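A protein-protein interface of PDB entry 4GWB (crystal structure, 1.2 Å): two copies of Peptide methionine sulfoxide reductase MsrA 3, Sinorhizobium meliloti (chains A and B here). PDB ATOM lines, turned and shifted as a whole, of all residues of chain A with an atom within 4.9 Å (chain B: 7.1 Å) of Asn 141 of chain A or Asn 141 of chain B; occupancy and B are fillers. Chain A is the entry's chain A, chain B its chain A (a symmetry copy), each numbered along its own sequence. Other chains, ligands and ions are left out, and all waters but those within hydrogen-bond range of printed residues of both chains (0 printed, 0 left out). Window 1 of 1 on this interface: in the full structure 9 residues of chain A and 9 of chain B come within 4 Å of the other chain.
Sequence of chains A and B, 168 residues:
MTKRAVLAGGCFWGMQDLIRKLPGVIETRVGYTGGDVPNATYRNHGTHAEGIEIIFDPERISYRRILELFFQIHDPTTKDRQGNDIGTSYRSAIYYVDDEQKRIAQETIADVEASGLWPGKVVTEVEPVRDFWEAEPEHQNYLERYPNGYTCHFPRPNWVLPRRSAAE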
ATOM      1  N   GLN A  16      14.954 -35.878  -5.303  1.00  0.00           N
ATOM      2  CA  GLN A  16      13.665 -35.207  -5.300  1.00  0.00           C
ATOM      3  C   GLN A  16      12.578 -36.104  -5.875  1.00  0.00           C
ATOM      4  O   GLN A  16      11.463 -36.150  -5.357  1.00  0.00           O
ATOM      5  CB  GLN A  16      13.738 -33.873  -6.032  1.00  0.00           C
ATOM      6  CG  GLN A  16      12.412 -33.140  -6.021  1.00  0.00           C
ATOM      7  CD  GLN A  16      12.457 -31.737  -6.591  1.00  0.00           C
ATOM      8  OE1 GLN A  16      13.184 -31.446  -7.548  1.00  0.00           O
ATOM      9  NE2 GLN A  16      11.650 -30.846  -6.014  1.00  0.00           N
ATOM     10  N   ARG A  20       9.780 -36.615  -2.899  1.00  0.00           N
ATOM     11  CA  ARG A  20       8.552 -35.850  -3.110  1.00  0.00           C
ATOM     12  C   ARG A  20       7.306 -36.742  -3.016  1.00  0.00           C
ATOM     13  O   ARG A  20       6.204 -36.221  -2.804  1.00  0.00           O
ATOM     14  CB  ARG A  20       8.567 -35.157  -4.468  1.00  0.00           C
ATOM     15  CG  ARG A  20       8.356 -36.108  -5.643  1.00  0.00           C
ATOM     16  CD  ARG A  20       8.616 -35.443  -6.988  1.00  0.00           C
ATOM     17  NE  ARG A  20       7.614 -34.397  -7.179  1.00  0.00           N
ATOM     18  CZ  ARG A  20       7.872 -33.144  -7.521  1.00  0.00           C
ATOM     19  NH1 ARG A  20       9.088 -32.763  -7.886  1.00  0.00           N
ATOM     20  NH2 ARG A  20       6.877 -32.259  -7.554  1.00  0.00           N
ATOM     21  N   HIS A 139      16.791 -27.197 -12.518  1.00  0.00           N
ATOM     22  CA  HIS A 139      16.981 -28.390 -11.688  1.00  0.00           C
ATOM     23  C   HIS A 139      15.783 -28.769 -10.840  1.00  0.00           C
ATOM     24  O   HIS A 139      15.711 -29.900 -10.383  1.00  0.00           O
ATOM     25  CB  HIS A 139      18.231 -28.246 -10.821  1.00  0.00           C
ATOM     26  CG  HIS A 139      19.466 -28.192 -11.629  1.00  0.00           C
ATOM     27  ND1 HIS A 139      19.875 -29.259 -12.388  1.00  0.00           N
ATOM     28  CD2 HIS A 139      20.334 -27.188 -11.864  1.00  0.00           C
ATOM     29  CE1 HIS A 139      20.961 -28.914 -13.053  1.00  0.00           C
ATOM     30  NE2 HIS A 139      21.259 -27.663 -12.753  1.00  0.00           N
ATOM     31  N   GLN A 140      14.870 -27.833 -10.604  1.00  0.00           N
ATOM     32  CA  GLN A 140      13.740 -28.100  -9.728  1.00  0.00           C
ATOM     33  C   GLN A 140      12.734 -28.971 -10.453  1.00  0.00           C
ATOM     34  O   GLN A 140      12.373 -28.675 -11.596  1.00  0.00           O
ATOM     35  CB  GLN A 140      13.075 -26.799  -9.268  1.00  0.00           C
ATOM     36  CG  GLN A 140      13.973 -25.791  -8.564  1.00  0.00           C
ATOM     37  CD  GLN A 140      14.672 -26.339  -7.334  1.00  0.00           C
ATOM     38  OE1 GLN A 140      14.161 -27.219  -6.642  1.00  0.00           O
ATOM     39  NE2 GLN A 140      15.846 -25.800  -7.046  1.00  0.00           N
ATOM     40  N   ASN A 141      12.287 -30.048  -9.815  1.00  0.00           N
ATOM     41  CA  ASN A 141      11.269 -30.932 -10.398  1.00  0.00           C
ATOM     42  C   ASN A 141      11.714 -31.519 -11.731  1.00  0.00           C
ATOM     43  O   ASN A 141      10.877 -31.793 -12.596  1.00  0.00           O
ATOM     44  CB  ASN A 141       9.925 -30.201 -10.562  1.00  0.00           C
ATOM     45  CG  ASN A 141       9.570 -29.423  -9.328  1.00  0.00           C
ATOM     46  OD1 ASN A 141       9.371 -30.012  -8.270  1.00  0.00           O
ATOM     47  ND2 ASN A 141       9.538 -28.099  -9.440  1.00  0.00           N
ATOM     48  N   TYR A 142      13.013 -31.747 -11.900  1.00  0.00           N
ATOM     49  CA  TYR A 142      13.536 -32.154 -13.190  1.00  0.00           C
ATOM     50  C   TYR A 142      12.871 -33.424 -13.700  1.00  0.00           C
ATOM     51  O   TYR A 142      12.441 -33.473 -14.858  1.00  0.00           O
ATOM     52  CB  TYR A 142      15.056 -32.319 -13.106  1.00  0.00           C
ATOM     53  CG  TYR A 142      15.661 -32.698 -14.415  1.00  0.00           C
ATOM     54  CD1 TYR A 142      15.854 -31.748 -15.403  1.00  0.00           C
ATOM     55  CD2 TYR A 142      15.979 -34.016 -14.681  1.00  0.00           C
ATOM     56  CE1 TYR A 142      16.391 -32.106 -16.621  1.00  0.00           C
ATOM     57  CE2 TYR A 142      16.527 -34.398 -15.883  1.00  0.00           C
ATOM     58  CZ  TYR A 142      16.726 -33.435 -16.853  1.00  0.00           C
ATOM     59  OH  TYR A 142      17.259 -33.811 -18.057  1.00  0.00           O
ATOM     60  N   LEU A 143      12.753 -34.450 -12.858  1.00  0.00           N
ATOM     61  CA  LEU A 143      12.196 -35.732 -13.276  1.00  0.00           C
ATOM     62  C   LEU A 143      10.664 -35.742 -13.326  1.00  0.00           C
ATOM     63  O   LEU A 143      10.085 -36.735 -13.742  1.00  0.00           O
ATOM     64  CB  LEU A 143      12.782 -36.884 -12.446  1.00  0.00           C
ATOM     65  CG  LEU A 143      14.296 -37.096 -12.629  1.00  0.00           C
ATOM     66  CD1 LEU A 143      14.840 -38.174 -11.711  1.00  0.00           C
ATOM     67  CD2 LEU A 143      14.656 -37.420 -14.073  1.00  0.00           C
ATOM     68  N   GLU A 144      10.022 -34.637 -12.959  1.00  0.00           N
ATOM     69  CA  GLU A 144       8.619 -34.424 -13.321  1.00  0.00           C
ATOM     70  C   GLU A 144       8.487 -33.985 -14.766  1.00  0.00           C
ATOM     71  O   GLU A 144       7.629 -34.481 -15.503  1.00  0.00           O
ATOM     72  CB  GLU A 144       7.977 -33.363 -12.430  1.00  0.00           C
ATOM     73  CG  GLU A 144       7.759 -33.810 -11.008  1.00  0.00           C
ATOM     74  CD  GLU A 144       6.795 -34.976 -10.919  1.00  0.00           C
ATOM     75  OE1 GLU A 144       5.604 -34.813 -11.260  1.00  0.00           O
ATOM     76  OE2 GLU A 144       7.223 -36.075 -10.531  1.00  0.00           O
ATOM     77  N   ARG A 145       9.327 -33.044 -15.171  1.00  0.00           N
ATOM     78  CA  ARG A 145       9.305 -32.562 -16.540  1.00  0.00           C
ATOM     79  C   ARG A 145       9.879 -33.593 -17.497  1.00  0.00           C
ATOM     80  O   ARG A 145       9.403 -33.709 -18.638  1.00  0.00           O
ATOM     81  CB  ARG A 145       9.988 -31.196 -16.641  1.00  0.00           C
ATOM     82  CG  ARG A 145       9.118 -30.126 -15.973  1.00  0.00           C
ATOM     83  CD  ARG A 145       9.738 -28.741 -15.927  1.00  0.00           C
ATOM     84  NE  ARG A 145      10.832 -28.668 -14.959  1.00  0.00           N
ATOM     85  CZ  ARG A 145      12.125 -28.645 -15.281  1.00  0.00           C
ATOM     86  NH1 ARG A 145      13.054 -28.557 -14.333  1.00  0.00           N
ATOM     87  NH2 ARG A 145      12.515 -28.752 -16.554  1.00  0.00           N
ATOM     88  N   TRP B  13      -0.099 -19.092 -14.703  1.00  0.00           N
ATOM     89  CA  TRP B  13       1.330 -18.796 -14.606  1.00  0.00           C
ATOM     90  C   TRP B  13       1.574 -17.558 -13.760  1.00  0.00           C
ATOM     91  O   TRP B  13       2.459 -17.545 -12.893  1.00  0.00           O
ATOM     92  CB  TRP B  13       1.943 -18.583 -15.976  1.00  0.00           C
ATOM     93  CG  TRP B  13       1.890 -19.743 -16.929  1.00  0.00           C
ATOM     94  CD1 TRP B  13       1.729 -21.077 -16.662  1.00  0.00           C
ATOM     95  CD2 TRP B  13       2.096 -19.640 -18.326  1.00  0.00           C
ATOM     96  NE1 TRP B  13       1.783 -21.814 -17.831  1.00  0.00           N
ATOM     97  CE2 TRP B  13       2.010 -20.948 -18.869  1.00  0.00           C
ATOM     98  CE3 TRP B  13       2.318 -18.558 -19.186  1.00  0.00           C
ATOM     99  CZ2 TRP B  13       2.153 -21.191 -20.235  1.00  0.00           C
ATOM    100  CZ3 TRP B  13       2.465 -18.803 -20.539  1.00  0.00           C
ATOM    101  CH2 TRP B  13       2.370 -20.107 -21.049  1.00  0.00           C
ATOM    102  N   GLN B  16       0.725 -18.055  -9.974  1.00  0.00           N
ATOM    103  CA  GLN B  16       1.757 -18.729  -9.204  1.00  0.00           C
ATOM    104  C   GLN B  16       2.970 -17.831  -9.008  1.00  0.00           C
ATOM    105  O   GLN B  16       3.552 -17.790  -7.925  1.00  0.00           O
ATOM    106  CB  GLN B  16       2.140 -20.058  -9.842  1.00  0.00           C
ATOM    107  CG  GLN B  16       3.196 -20.794  -9.043  1.00  0.00           C
ATOM    108  CD  GLN B  16       3.505 -22.193  -9.536  1.00  0.00           C
ATOM    109  OE1 GLN B  16       3.497 -22.477 -10.740  1.00  0.00           O
ATOM    110  NE2 GLN B  16       3.808 -23.090  -8.596  1.00  0.00           N
ATOM    111  N   ASP B  17       3.344 -17.077 -10.036  1.00  0.00           N
ATOM    112  CA  ASP B  17       4.520 -16.211  -9.974  1.00  0.00           C
ATOM    113  C   ASP B  17       4.448 -15.248  -8.794  1.00  0.00           C
ATOM    114  O   ASP B  17       5.470 -15.011  -8.131  1.00  0.00           O
ATOM    115  CB  ASP B  17       4.623 -15.440 -11.305  1.00  0.00           C
ATOM    116  CG  ASP B  17       5.761 -14.462 -11.368  1.00  0.00           C
ATOM    117  OD1 ASP B  17       6.904 -14.831 -11.066  1.00  0.00           O
ATOM    118  OD2 ASP B  17       5.490 -13.312 -11.803  1.00  0.00           O
ATOM    119  N   ARG B  20       3.427 -17.344  -4.946  1.00  0.00           N
ATOM    120  CA  ARG B  20       4.539 -18.110  -4.384  1.00  0.00           C
ATOM    121  C   ARG B  20       5.478 -17.221  -3.557  1.00  0.00           C
ATOM    122  O   ARG B  20       6.235 -17.746  -2.731  1.00  0.00           O
ATOM    123  CB  ARG B  20       5.341 -18.794  -5.485  1.00  0.00           C
ATOM    124  CG  ARG B  20       6.212 -17.836  -6.293  1.00  0.00           C
ATOM    125  CD  ARG B  20       6.811 -18.493  -7.529  1.00  0.00           C
ATOM    126  NE  ARG B  20       7.729 -19.540  -7.089  1.00  0.00           N
ATOM    127  CZ  ARG B  20       7.730 -20.790  -7.526  1.00  0.00           C
ATOM    128  NH1 ARG B  20       6.976 -21.166  -8.548  1.00  0.00           N
ATOM    129  NH2 ARG B  20       8.548 -21.677  -6.961  1.00  0.00           N
ATOM    130  N   GLU B  27       4.008 -24.145  -0.497  1.00  0.00           N
ATOM    131  CA  GLU B  27       3.981 -24.780  -1.810  1.00  0.00           C
ATOM    132  C   GLU B  27       2.834 -24.204  -2.587  1.00  0.00           C
ATOM    133  O   GLU B  27       1.801 -23.835  -2.026  1.00  0.00           O
ATOM    134  CB  GLU B  27       3.843 -26.313  -1.690  1.00  0.00           C
ATOM    135  CG  GLU B  27       3.660 -27.101  -2.998  1.00  0.00           C
ATOM    136  CD  GLU B  27       4.776 -26.943  -4.034  1.00  0.00           C
ATOM    137  OE1 GLU B  27       5.464 -25.910  -4.062  1.00  0.00           O
ATOM    138  OE2 GLU B  27       5.004 -27.877  -4.858  1.00  0.00           O
ATOM    139  N   THR B  28       3.017 -24.130  -3.897  1.00  0.00           N
ATOM    140  CA  THR B  28       1.959 -23.783  -4.815  1.00  0.00           C
ATOM    141  C   THR B  28       1.985 -24.785  -5.961  1.00  0.00           C
ATOM    142  O   THR B  28       3.066 -25.242  -6.372  1.00  0.00           O
ATOM    143  CB  THR B  28       2.153 -22.355  -5.382  1.00  0.00           C
ATOM    144  OG1 THR B  28       3.475 -22.192  -5.917  1.00  0.00           O
ATOM    145  CG2 THR B  28       1.899 -21.283  -4.340  1.00  0.00           C
ATOM    146  N   ARG B  29       0.803 -25.104  -6.483  1.00  0.00           N
ATOM    147  CA  ARG B  29       0.714 -25.889  -7.703  1.00  0.00           C
ATOM    148  C   ARG B  29      -0.478 -25.407  -8.496  1.00  0.00           C
ATOM    149  O   ARG B  29      -1.504 -24.993  -7.939  1.00  0.00           O
ATOM    150  CB  ARG B  29       0.645 -27.377  -7.464  1.00  0.00           C
ATOM    151  CG  ARG B  29      -0.549 -27.805  -6.720  1.00  0.00           C
ATOM    152  CD  ARG B  29      -0.652 -29.328  -6.683  1.00  0.00           C
ATOM    153  NE  ARG B  29      -1.812 -29.736  -5.891  1.00  0.00           N
ATOM    154  CZ  ARG B  29      -2.572 -30.807  -6.117  1.00  0.00           C
ATOM    155  NH1 ARG B  29      -2.316 -31.633  -7.120  1.00  0.00           N
ATOM    156  NH2 ARG B  29      -3.609 -31.047  -5.323  1.00  0.00           N
ATOM    157  N   VAL B  30      -0.340 -25.425  -9.812  1.00  0.00           N
ATOM    158  CA  VAL B  30      -1.405 -24.920 -10.678  1.00  0.00           C
ATOM    159  C   VAL B  30      -2.167 -26.109 -11.261  1.00  0.00           C
ATOM    160  O   VAL B  30      -1.653 -27.230 -11.321  1.00  0.00           O
ATOM    161  CB  VAL B  30      -0.885 -23.936 -11.759  1.00  0.00           C
ATOM    162  CG1 VAL B  30      -0.220 -22.746 -11.090  1.00  0.00           C
ATOM    163  CG2 VAL B  30       0.062 -24.614 -12.757  1.00  0.00           C
ATOM    164  N   PRO B 137       3.369 -31.025 -15.923  1.00  0.00           N
ATOM    165  CA  PRO B 137       4.619 -30.492 -15.352  1.00  0.00           C
ATOM    166  C   PRO B 137       5.122 -29.226 -16.016  1.00  0.00           C
ATOM    167  O   PRO B 137       5.645 -28.341 -15.327  1.00  0.00           O
ATOM    168  CB  PRO B 137       5.614 -31.644 -15.543  1.00  0.00           C
ATOM    169  CG  PRO B 137       4.749 -32.860 -15.511  1.00  0.00           C
ATOM    170  CD  PRO B 137       3.477 -32.467 -16.211  1.00  0.00           C
ATOM    171  N   GLU B 138       4.937 -29.087 -17.331  1.00  0.00           N
ATOM    172  CA  GLU B 138       5.400 -27.887 -18.029  1.00  0.00           C
ATOM    173  C   GLU B 138       4.783 -26.599 -17.503  1.00  0.00           C
ATOM    174  O   GLU B 138       5.375 -25.533 -17.630  1.00  0.00           O
ATOM    175  CB  GLU B 138       5.196 -27.982 -19.551  1.00  0.00           C
ATOM    176  CG  GLU B 138       3.767 -28.180 -20.012  1.00  0.00           C
ATOM    177  CD  GLU B 138       3.384 -29.642 -20.181  1.00  0.00           C
ATOM    178  OE1 GLU B 138       2.428 -29.897 -20.953  1.00  0.00           O
ATOM    179  OE2 GLU B 138       4.018 -30.532 -19.558  1.00  0.00           O
ATOM    180  N   HIS B 139       3.594 -26.688 -16.906  1.00  0.00           N
ATOM    181  CA  HIS B 139       2.941 -25.499 -16.347  1.00  0.00           C
ATOM    182  C   HIS B 139       3.392 -25.128 -14.949  1.00  0.00           C
ATOM    183  O   HIS B 139       3.174 -24.000 -14.532  1.00  0.00           O
ATOM    184  CB  HIS B 139       1.422 -25.645 -16.403  1.00  0.00           C
ATOM    185  CG  HIS B 139       0.917 -25.692 -17.790  1.00  0.00           C
ATOM    186  ND1 HIS B 139       1.042 -24.620 -18.636  1.00  0.00           N
ATOM    187  CD2 HIS B 139       0.365 -26.693 -18.504  1.00  0.00           C
ATOM    188  CE1 HIS B 139       0.572 -24.958 -19.821  1.00  0.00           C
ATOM    189  NE2 HIS B 139       0.155 -26.211 -19.767  1.00  0.00           N
ATOM    190  N   GLN B 140       3.984 -26.067 -14.218  1.00  0.00           N
ATOM    191  CA  GLN B 140       4.364 -25.808 -12.838  1.00  0.00           C
ATOM    192  C   GLN B 140       5.601 -24.935 -12.811  1.00  0.00           C
ATOM    193  O   GLN B 140       6.576 -25.224 -13.512  1.00  0.00           O
ATOM    194  CB  GLN B 140       4.624 -27.113 -12.080  1.00  0.00           C
ATOM    195  CG  GLN B 140       3.484 -28.124 -12.060  1.00  0.00           C
ATOM    196  CD  GLN B 140       2.187 -27.582 -11.491  1.00  0.00           C
ATOM    197  OE1 GLN B 140       2.180 -26.707 -10.625  1.00  0.00           O
ATOM    198  NE2 GLN B 140       1.076 -28.120 -11.967  1.00  0.00           N
ATOM    199  N   ASN B 141       5.575 -23.862 -12.026  1.00  0.00           N
ATOM    200  CA  ASN B 141       6.738 -22.977 -11.877  1.00  0.00           C
ATOM    201  C   ASN B 141       7.179 -22.381 -13.208  1.00  0.00           C
ATOM    202  O   ASN B 141       8.366 -22.103 -13.397  1.00  0.00           O
ATOM    203  CB  ASN B 141       7.914 -23.709 -11.208  1.00  0.00           C
ATOM    204  CG  ASN B 141       7.461 -24.496 -10.013  1.00  0.00           C
ATOM    205  OD1 ASN B 141       6.985 -23.914  -9.042  1.00  0.00           O
ATOM    206  ND2 ASN B 141       7.557 -25.819 -10.091  1.00  0.00           N
ATOM    207  N   TYR B 142       6.239 -22.149 -14.120  1.00  0.00           N
ATOM    208  CA  TYR B 142       6.593 -21.733 -15.463  1.00  0.00           C
ATOM    209  C   TYR B 142       7.428 -20.461 -15.466  1.00  0.00           C
ATOM    210  O   TYR B 142       8.465 -20.406 -16.135  1.00  0.00           O
ATOM    211  CB  TYR B 142       5.325 -21.565 -16.305  1.00  0.00           C
ATOM    212  CG  TYR B 142       5.623 -21.177 -17.714  1.00  0.00           C
ATOM    213  CD1 TYR B 142       6.062 -22.120 -18.627  1.00  0.00           C
ATOM    214  CD2 TYR B 142       5.525 -19.856 -18.110  1.00  0.00           C
ATOM    215  CE1 TYR B 142       6.361 -21.754 -19.922  1.00  0.00           C
ATOM    216  CE2 TYR B 142       5.806 -19.466 -19.398  1.00  0.00           C
ATOM    217  CZ  TYR B 142       6.229 -20.422 -20.299  1.00  0.00           C
ATOM    218  OH  TYR B 142       6.523 -20.038 -21.581  1.00  0.00           O
ATOM    219  N   LEU B 143       7.015 -19.441 -14.714  1.00  0.00           N
ATOM    220  CA  LEU B 143       7.709 -18.157 -14.708  1.00  0.00           C
ATOM    221  C   LEU B 143       8.967 -18.150 -13.830  1.00  0.00           C
ATOM    222  O   LEU B 143       9.677 -17.155 -13.809  1.00  0.00           O
ATOM    223  CB  LEU B 143       6.741 -17.009 -14.387  1.00  0.00           C
ATOM    224  CG  LEU B 143       5.637 -16.793 -15.439  1.00  0.00           C
ATOM    225  CD1 LEU B 143       4.650 -15.720 -15.022  1.00  0.00           C
ATOM    226  CD2 LEU B 143       6.213 -16.459 -16.809  1.00  0.00           C
ATOM    227  N   GLU B 144       9.263 -19.258 -13.158  1.00  0.00           N
ATOM    228  CA  GLU B 144      10.604 -19.472 -12.609  1.00  0.00           C
ATOM    229  C   GLU B 144      11.576 -19.903 -13.690  1.00  0.00           C
ATOM    230  O   GLU B 144      12.703 -19.404 -13.764  1.00  0.00           O
ATOM    231  CB  GLU B 144      10.586 -20.540 -11.517  1.00  0.00           C
ATOM    232  CG  GLU B 144       9.908 -20.103 -10.246  1.00  0.00           C
ATOM    233  CD  GLU B 144      10.624 -18.938  -9.590  1.00  0.00           C
ATOM    234  OE1 GLU B 144      11.783 -19.102  -9.150  1.00  0.00           O
ATOM    235  OE2 GLU B 144      10.047 -17.842  -9.529  1.00  0.00           O
ATOM    236  N   ARG B 145      11.147 -20.839 -14.523  1.00  0.00           N
ATOM    237  CA  ARG B 145      11.986 -21.313 -15.609  1.00  0.00           C
ATOM    238  C   ARG B 145      12.098 -20.275 -16.713  1.00  0.00           C
ATOM    239  O   ARG B 145      13.161 -20.153 -17.341  1.00  0.00           O
ATOM    240  CB  ARG B 145      11.503 -22.677 -16.108  1.00  0.00           C
ATOM    241  CG  ARG B 145      11.801 -23.752 -15.059  1.00  0.00           C
ATOM    242  CD  ARG B 145      11.280 -25.136 -15.402  1.00  0.00           C
ATOM    243  NE  ARG B 145       9.824 -25.213 -15.283  1.00  0.00           N
ATOM    244  CZ  ARG B 145       8.982 -25.232 -16.314  1.00  0.00           C
ATOM    245  NH1 ARG B 145       7.670 -25.324 -16.112  1.00  0.00           N
ATOM    246  NH2 ARG B 145       9.432 -25.116 -17.567  1.00  0.00           N
ATOM    247  N   TYR B 146      11.033 -19.494 -16.918  1.00  0.00           N
ATOM    248  CA  TYR B 146      10.984 -18.439 -17.942  1.00  0.00           C
ATOM    249  C   TYR B 146      10.612 -17.120 -17.299  1.00  0.00           C
ATOM    250  O   TYR B 146       9.461 -16.679 -17.391  1.00  0.00           O
ATOM    251  CB  TYR B 146       9.984 -18.830 -19.011  1.00  0.00           C
ATOM    252  CG  TYR B 146      10.437 -20.029 -19.770  1.00  0.00           C
ATOM    253  CD1 TYR B 146      11.418 -19.895 -20.751  1.00  0.00           C
ATOM    254  CD2 TYR B 146       9.927 -21.294 -19.507  1.00  0.00           C
ATOM    255  CE1 TYR B 146      11.866 -20.987 -21.455  1.00  0.00           C
ATOM    256  CE2 TYR B 146      10.371 -22.403 -20.216  1.00  0.00           C
ATOM    257  CZ  TYR B 146      11.338 -22.231 -21.190  1.00  0.00           C
ATOM    258  OH  TYR B 146      11.807 -23.297 -21.913  1.00  0.00           O
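Asn 141 of chain B touches its own counterpart, Asn 141 of chain A. Arg 145 of chain B touches its own counterpart, Arg 145 of chain A.
Along chain A the printed residues that touch a printed residue of chain B span positions 141 to 145. Hydrophobic or aromatic side chains of chain B within 4 Å of the printed part of chain A: Pro 137.
The side-chain amide nitrogen (ND2) of Asn 141 of chain A sits close to the side-chain amide nitrogen (ND2) of Asn 141 of chain B, 3.1 Å away.
Printed residues of chain B within 4 Å of Glu 144 of chain A: Pro 137 (3.3 Å). Printed residues of chain B within 4 Å of Arg 145 of chain A: Pro 137 and Arg 145. Of the printed residues of chain A, Pro 137 of chain B touches Glu 144 and Arg 145. Of chain A, only Asn 141 (3.1 Å) comes within 4 Å of Asn 141 of chain B. Of the printed residues of chain A, Arg 145 of chain B touches Arg 145 (3.6 Å). The nearest printed residue of chain A that does not touch Asn 141 of chain B is Gln 140 of chain A (5.7 Å). The nearest printed residue of chain B that does not touch Glu 144 of chain A is Glu 138 of chain B (6.3 Å).
O of Glu 138 of chain B sits at hydrogen-bond distance from NH1 of Arg 145 of chain B, at 2.8 Å. OE1 of Gln 16 of chain A lies within hydrogen-bond range of N of Asn 141 of chain A (2.8 Å). The guanidinium group of Arg 20 of chain A is in salt-bridge range of the side-chain carboxylate of Glu 144 of chain A. NH1 of Arg 20 of chain B is in hydrogen-bond range of OD1 of Asn 141 of chain B (2.8 Å). OE1 of Gln 16 of chain B sits at hydrogen-bond distance from N of Asn 141 of chain B. The backbone carbonyl oxygen of Gln 140 of chain B lies within hydrogen-bond range of the guanidinium group of Arg 145 of chain B, 2.8 Å away.
Among the printed residues, merely in contact across the chains: Glu 144 of chain A with Pro 137 of chain B (3.3 Å), Arg 145 of chain A with Arg 145 of chain B (3.6 Å) and Arg 145 of chain A with Pro 137 of chain B (3.8 Å).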
